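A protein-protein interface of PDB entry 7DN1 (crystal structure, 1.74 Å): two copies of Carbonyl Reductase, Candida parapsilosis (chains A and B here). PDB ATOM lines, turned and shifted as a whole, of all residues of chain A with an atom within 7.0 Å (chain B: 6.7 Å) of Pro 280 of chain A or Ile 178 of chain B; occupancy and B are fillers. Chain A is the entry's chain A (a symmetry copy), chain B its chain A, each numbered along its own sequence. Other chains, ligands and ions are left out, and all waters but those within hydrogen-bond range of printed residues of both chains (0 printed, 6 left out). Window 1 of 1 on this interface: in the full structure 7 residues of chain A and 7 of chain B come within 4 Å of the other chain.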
ATOM      1  N   LEU A 239      28.925   1.647  18.171  1.00  0.00           N
ATOM      2  CA  LEU A 239      28.509   2.879  17.527  1.00  0.00           C
ATOM      3  C   LEU A 239      27.014   2.903  17.227  1.00  0.00           C
ATOM      4  O   LEU A 239      26.519   3.901  16.702  1.00  0.00           O
ATOM      5  CB  LEU A 239      29.328   3.069  16.242  1.00  0.00           C
ATOM      6  CG  LEU A 239      30.735   3.676  16.455  1.00  0.00           C
ATOM      7  CD1 LEU A 239      30.596   5.072  17.039  1.00  0.00           C
ATOM      8  CD2 LEU A 239      31.595   2.869  17.350  1.00  0.00           C
ATOM      9  N   THR A 240      26.288   1.836  17.575  1.00  0.00           N
ATOM     10  CA  THR A 240      24.847   1.736  17.351  1.00  0.00           C
ATOM     11  C   THR A 240      24.118   2.090  18.635  1.00  0.00           C
ATOM     12  O   THR A 240      24.284   1.368  19.630  1.00  0.00           O
ATOM     13  CB  THR A 240      24.471   0.315  16.937  1.00  0.00           C
ATOM     14  OG1 THR A 240      25.233  -0.077  15.785  1.00  0.00           O
ATOM     15  CG2 THR A 240      22.940   0.227  16.617  1.00  0.00           C
ATOM     16  N   PRO A 241      23.292   3.142  18.668  1.00  0.00           N
ATOM     17  CA  PRO A 241      22.605   3.504  19.923  1.00  0.00           C
ATOM     18  C   PRO A 241      21.848   2.373  20.596  1.00  0.00           C
ATOM     19  O   PRO A 241      21.825   2.321  21.834  1.00  0.00           O
ATOM     20  CB  PRO A 241      21.661   4.625  19.473  1.00  0.00           C
ATOM     21  CG  PRO A 241      22.479   5.319  18.441  1.00  0.00           C
ATOM     22  CD  PRO A 241      23.091   4.188  17.638  1.00  0.00           C
ATOM     23  N   GLY A 275      18.682   1.143  14.240  1.00  0.00           N
ATOM     24  CA  GLY A 275      19.083   1.151  15.640  1.00  0.00           C
ATOM     25  C   GLY A 275      19.671   2.471  16.082  1.00  0.00           C
ATOM     26  O   GLY A 275      20.339   2.537  17.121  1.00  0.00           O
ATOM     27  N   GLY A 276      19.422   3.532  15.316  1.00  0.00           N
ATOM     28  CA  GLY A 276      19.943   4.845  15.624  1.00  0.00           C
ATOM     29  C   GLY A 276      21.309   5.142  15.054  1.00  0.00           C
ATOM     30  O   GLY A 276      21.868   6.192  15.372  1.00  0.00           O
ATOM     31  N   TYR A 277      21.853   4.261  14.213  1.00  0.00           N
ATOM     32  CA  TYR A 277      23.254   4.371  13.811  1.00  0.00           C
ATOM     33  C   TYR A 277      23.558   5.715  13.151  1.00  0.00           C
ATOM     34  O   TYR A 277      24.662   6.261  13.321  1.00  0.00           O
ATOM     35  CB  TYR A 277      23.624   3.213  12.882  1.00  0.00           C
ATOM     36  CG  TYR A 277      25.104   3.148  12.620  1.00  0.00           C
ATOM     37  CD1 TYR A 277      25.690   3.974  11.679  1.00  0.00           C
ATOM     38  CD2 TYR A 277      25.927   2.303  13.354  1.00  0.00           C
ATOM     39  CE1 TYR A 277      27.047   3.957  11.461  1.00  0.00           C
ATOM     40  CE2 TYR A 277      27.302   2.283  13.124  1.00  0.00           C
ATOM     41  CZ  TYR A 277      27.841   3.110  12.159  1.00  0.00           C
ATOM     42  OH  TYR A 277      29.203   3.111  11.912  1.00  0.00           O
ATOM     43  N   THR A 278      22.609   6.262  12.395  1.00  0.00           N
ATOM     44  CA  THR A 278      22.894   7.518  11.710  1.00  0.00           C
ATOM     45  C   THR A 278      22.844   8.732  12.631  1.00  0.00           C
ATOM     46  O   THR A 278      23.223   9.824  12.199  1.00  0.00           O
ATOM     47  CB  THR A 278      21.941   7.710  10.525  1.00  0.00           C
ATOM     48  OG1 THR A 278      20.582   7.561  10.952  1.00  0.00           O
ATOM     49  CG2 THR A 278      22.244   6.657   9.468  1.00  0.00           C
ATOM     50  N   CYS A 279      22.418   8.579  13.883  1.00  0.00           N
ATOM     51  CA  CYS A 279      22.310   9.745  14.753  1.00  0.00           C
ATOM     52  C   CYS A 279      23.647  10.255  15.293  1.00  0.00           C
ATOM     53  O   CYS A 279      23.894  11.468  15.233  1.00  0.00           O
ATOM     54  CB  CYS A 279      21.345   9.450  15.893  1.00  0.00           C
ATOM     55  SG  CYS A 279      19.679   9.213  15.274  1.00  0.00           S
ATOM     56  N   PRO A 280      24.535   9.401  15.853  1.00  0.00           N
ATOM     57  CA  PRO A 280      25.839   9.928  16.275  1.00  0.00           C
ATOM     58  C   PRO A 280      26.706  10.342  15.077  1.00  0.00           C
ATOM     59  O   PRO A 280      27.859  10.785  15.253  1.00  0.00           O
ATOM     60  CB  PRO A 280      26.481   8.754  17.038  1.00  0.00           C
ATOM     61  CG  PRO A 280      25.375   7.721  17.215  1.00  0.00           C
ATOM     62  CD  PRO A 280      24.421   7.957  16.092  1.00  0.00           C
ATOM     63  N   SER B 173      27.191  24.170  15.046  1.00  0.00           N
ATOM     64  CA  SER B 173      28.061  23.123  15.562  1.00  0.00           C
ATOM     65  C   SER B 173      27.700  21.877  14.784  1.00  0.00           C
ATOM     66  O   SER B 173      26.584  21.773  14.269  1.00  0.00           O
ATOM     67  CB  SER B 173      27.853  22.898  17.061  1.00  0.00           C
ATOM     68  OG  SER B 173      28.470  21.710  17.489  1.00  0.00           O
ATOM     69  N   ILE B 174      28.629  20.921  14.719  1.00  0.00           N
ATOM     70  CA  ILE B 174      28.208  19.609  14.245  1.00  0.00           C
ATOM     71  C   ILE B 174      27.125  19.043  15.148  1.00  0.00           C
ATOM     72  O   ILE B 174      26.369  18.179  14.712  1.00  0.00           O
ATOM     73  CB  ILE B 174      29.395  18.620  14.090  1.00  0.00           C
ATOM     74  CG1 ILE B 174      30.198  18.417  15.367  1.00  0.00           C
ATOM     75  CG2 ILE B 174      30.312  19.047  12.958  1.00  0.00           C
ATOM     76  CD1 ILE B 174      31.230  17.264  15.183  1.00  0.00           C
ATOM     77  N   SER B 175      26.991  19.558  16.374  1.00  0.00           N
ATOM     78  CA  SER B 175      25.949  19.103  17.293  1.00  0.00           C
ATOM     79  C   SER B 175      24.544  19.416  16.808  1.00  0.00           C
ATOM     80  O   SER B 175      23.579  18.852  17.349  1.00  0.00           O
ATOM     81  CB  SER B 175      26.140  19.728  18.675  1.00  0.00           C
ATOM     82  OG  SER B 175      27.405  19.391  19.220  1.00  0.00           O
ATOM     83  N   GLY B 176      24.408  20.298  15.821  1.00  0.00           N
ATOM     84  CA  GLY B 176      23.137  20.555  15.188  1.00  0.00           C
ATOM     85  C   GLY B 176      22.764  19.548  14.130  1.00  0.00           C
ATOM     86  O   GLY B 176      21.618  19.553  13.669  1.00  0.00           O
ATOM     87  N   LYS B 177      23.719  18.710  13.724  1.00  0.00           N
ATOM     88  CA  LYS B 177      23.540  17.687  12.700  1.00  0.00           C
ATOM     89  C   LYS B 177      23.639  16.275  13.246  1.00  0.00           C
ATOM     90  O   LYS B 177      22.923  15.388  12.773  1.00  0.00           O
ATOM     91  CB  LYS B 177      24.588  17.842  11.580  1.00  0.00           C
ATOM     92  CG  LYS B 177      24.736  19.242  10.977  1.00  0.00           C
ATOM     93  CD  LYS B 177      23.440  19.768  10.410  1.00  0.00           C
ATOM     94  CE  LYS B 177      23.011  19.048   9.138  1.00  0.00           C
ATOM     95  NZ  LYS B 177      21.571  19.316   8.855  1.00  0.00           N
ATOM     96  N   ILE B 178      24.541  16.051  14.210  1.00  0.00           N
ATOM     97  CA  ILE B 178      24.759  14.745  14.830  1.00  0.00           C
ATOM     98  C   ILE B 178      24.499  14.825  16.323  1.00  0.00           C
ATOM     99  O   ILE B 178      24.351  15.913  16.885  1.00  0.00           O
ATOM    100  CB  ILE B 178      26.196  14.249  14.678  1.00  0.00           C
ATOM    101  CG1 ILE B 178      27.057  15.249  15.468  1.00  0.00           C
ATOM    102  CG2 ILE B 178      26.543  14.115  13.201  1.00  0.00           C
ATOM    103  CD1 ILE B 178      28.408  14.911  15.689  1.00  0.00           C
ATOM    104  N   VAL B 179      24.542  13.668  16.989  1.00  0.00           N
ATOM    105  CA  VAL B 179      24.376  13.569  18.431  1.00  0.00           C
ATOM    106  C   VAL B 179      25.754  13.223  18.993  1.00  0.00           C
ATOM    107  O   VAL B 179      26.293  12.146  18.711  1.00  0.00           O
ATOM    108  CB  VAL B 179      23.320  12.518  18.805  1.00  0.00           C
ATOM    109  CG1 VAL B 179      23.139  12.408  20.320  1.00  0.00           C
ATOM    110  CG2 VAL B 179      21.967  12.878  18.142  1.00  0.00           C
ATOM    111  N   ASN B 180      26.345  14.148  19.749  1.00  0.00           N
ATOM    112  CA  ASN B 180      27.662  13.879  20.325  1.00  0.00           C
ATOM    113  C   ASN B 180      27.642  12.688  21.271  1.00  0.00           C
ATOM    114  O   ASN B 180      26.676  12.465  22.009  1.00  0.00           O
ATOM    115  CB  ASN B 180      28.208  15.093  21.072  1.00  0.00           C
ATOM    116  CG  ASN B 180      28.286  16.313  20.206  1.00  0.00           C
ATOM    117  OD1 ASN B 180      27.272  16.851  19.768  1.00  0.00           O
ATOM    118  ND2 ASN B 180      29.502  16.724  19.900  1.00  0.00           N
ATOM    119  N   ILE B 181      28.739  11.931  21.241  1.00  0.00           N
ATOM    120  CA  ILE B 181      28.992  10.809  22.149  1.00  0.00           C
ATOM    121  C   ILE B 181      30.471  10.788  22.488  1.00  0.00           C
ATOM    122  O   ILE B 181      31.320  11.183  21.677  1.00  0.00           O
ATOM    123  CB  ILE B 181      28.586   9.462  21.515  1.00  0.00           C
ATOM    124  CG1 ILE B 181      29.288   9.277  20.169  1.00  0.00           C
ATOM    125  CG2 ILE B 181      27.072   9.365  21.342  1.00  0.00           C
ATOM    126  CD1 ILE B 181      29.398   7.842  19.695  1.00  0.00           C
ATOM    127  N   ASN B 189      22.595  20.161  21.661  1.00  0.00           N
ATOM    128  CA  ASN B 189      22.305  19.705  20.300  1.00  0.00           C
ATOM    129  C   ASN B 189      21.017  20.326  19.769  1.00  0.00           C
ATOM    130  O   ASN B 189      20.948  20.758  18.606  1.00  0.00           O
ATOM    131  CB  ASN B 189      22.199  18.178  20.267  1.00  0.00           C
ATOM    132  CG  ASN B 189      23.432  17.490  20.841  1.00  0.00           C
ATOM    133  OD1 ASN B 189      24.502  18.095  20.967  1.00  0.00           O
ATOM    134  ND2 ASN B 189      23.288  16.207  21.192  1.00  0.00           N
ATOM    135  N   TYR B 219      35.122  19.355  16.676  1.00  0.00           N
ATOM    136  CA  TYR B 219      35.857  19.543  17.924  1.00  0.00           C
ATOM    137  C   TYR B 219      37.063  20.444  17.683  1.00  0.00           C
ATOM    138  O   TYR B 219      37.976  20.073  16.942  1.00  0.00           O
ATOM    139  CB  TYR B 219      36.287  18.190  18.489  1.00  0.00           C
ATOM    140  CG  TYR B 219      35.116  17.379  18.999  1.00  0.00           C
ATOM    141  CD1 TYR B 219      34.412  17.788  20.131  1.00  0.00           C
ATOM    142  CD2 TYR B 219      34.708  16.212  18.352  1.00  0.00           C
ATOM    143  CE1 TYR B 219      33.320  17.067  20.604  1.00  0.00           C
ATOM    144  CE2 TYR B 219      33.611  15.478  18.826  1.00  0.00           C
ATOM    145  CZ  TYR B 219      32.927  15.922  19.949  1.00  0.00           C
ATOM    146  OH  TYR B 219      31.851  15.224  20.440  1.00  0.00           O
ATOM    147  N   TYR B 277      33.963  14.611  10.710  1.00  0.00           N
ATOM    148  CA  TYR B 277      33.272  13.897  11.782  1.00  0.00           C
ATOM    149  C   TYR B 277      31.849  13.503  11.386  1.00  0.00           C
ATOM    150  O   TYR B 277      31.357  12.437  11.794  1.00  0.00           O
ATOM    151  CB  TYR B 277      33.268  14.743  13.057  1.00  0.00           C
ATOM    152  CG  TYR B 277      32.774  13.969  14.248  1.00  0.00           C
ATOM    153  CD1 TYR B 277      31.419  13.796  14.464  1.00  0.00           C
ATOM    154  CD2 TYR B 277      33.660  13.359  15.127  1.00  0.00           C
ATOM    155  CE1 TYR B 277      30.954  13.055  15.524  1.00  0.00           C
ATOM    156  CE2 TYR B 277      33.185  12.615  16.206  1.00  0.00           C
ATOM    157  CZ  TYR B 277      31.823  12.487  16.395  1.00  0.00           C
ATOM    158  OH  TYR B 277      31.324  11.752  17.456  1.00  0.00           O
ATOM    159  N   THR B 278      31.170  14.342  10.607  1.00  0.00           N
ATOM    160  CA  THR B 278      29.791  14.016  10.260  1.00  0.00           C
ATOM    161  C   THR B 278      29.677  12.942   9.184  1.00  0.00           C
ATOM    162  O   THR B 278      28.565  12.473   8.925  1.00  0.00           O
ATOM    163  CB  THR B 278      29.035  15.279   9.832  1.00  0.00           C
ATOM    164  OG1 THR B 278      29.758  15.968   8.806  1.00  0.00           O
ATOM    165  CG2 THR B 278      28.885  16.201  11.034  1.00  0.00           C
ATOM    166  N   CYS B 279      30.781  12.518   8.571  1.00  0.00           N
ATOM    167  CA  CYS B 279      30.675  11.534   7.500  1.00  0.00           C
ATOM    168  C   CYS B 279      30.419  10.105   7.980  1.00  0.00           C
ATOM    169  O   CYS B 279      29.528   9.440   7.432  1.00  0.00           O
ATOM    170  CB  CYS B 279      31.917  11.594   6.620  1.00  0.00           C
ATOM    171  SG  CYS B 279      32.016  13.164   5.761  1.00  0.00           S
ATOM    172  N   PRO B 280      31.170   9.564   8.966  1.00  0.00           N
ATOM    173  CA  PRO B 280      30.826   8.220   9.449  1.00  0.00           C
ATOM    174  C   PRO B 280      29.487   8.207  10.203  1.00  0.00           C
ATOM    175  O   PRO B 280      29.056   7.151  10.707  1.00  0.00           O
ATOM    176  CB  PRO B 280      31.990   7.858  10.390  1.00  0.00           C
ATOM    177  CG  PRO B 280      33.050   8.930  10.170  1.00  0.00           C
ATOM    178  CD  PRO B 280      32.310  10.136   9.695  1.00  0.00           C
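Of the printed residues of chain B, Tyr 277 of chain A touches Pro 280 (3.8 Å).
Of the printed residues of chain B, Cys 279 of chain A touches Ile 178 and Val 179.
Pro 280 of chain A touches just these residues of chain B: Ile 178 (3.9 Å), Val 179 (3.3 Å) and Tyr 277 (3.8 Å).
Lys 177 of chain B touches none of the printed residues of chain A.
Of the printed residues of chain A, Val 179 of chain B touches Cys 279 (2.9 Å) and Pro 280 (3.3 Å).
Of the printed residues of chain A, Tyr 277 of chain B touches Pro 280 (3.8 Å).
Printed residues of chain A within 4 Å of Pro 280 of chain B: Tyr 277.
The nearest printed residue of chain A that does not touch Pro 280 of chain B is Pro 280 of chain A (5.9 Å).
CE1 of Tyr 277 of chain A touches O of Pro 280 of chain B, 3.8 Å away.
O of Cys 279 of chain A touches CA of Ile 178 of chain B (3.4 Å).
Pro 280 of chain A touches Ile 178 of chain B.
Val 179 of chain B touches Pro 280 of chain A (O to CA, 3.3 Å).
Pro 280 of chain A touches Tyr 277 of chain B (O to CE1, 3.8 Å).
Tyr 277 of chain A touches Pro 280 of chain B, and with the chains exchanged Pro 280 of chain A touches Tyr 277 of chain B.
The backbone carbonyl oxygen of Cys 279 of chain A is in hydrogen-bond range of the backbone NH of Val 179 of chain B, 2.9 Å away.
O of Gly 276 of chain A lies close to SG of Cys 279 of chain A (3.7 Å).
Of the 15 printed residues of chain B, 4 touch a printed residue of chain A.
Printed residues of chain B that touch a printed residue of chain A: Ile 178, Val 179, Tyr 277 and Pro 280.
Hydrophobic or aromatic side chains of chain B within 4 Å of the printed part of chain A: Ile 178, Val 179 and Tyr 277.
Of the 9 printed residues of chain A, 3 touch a printed residue of chain B.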
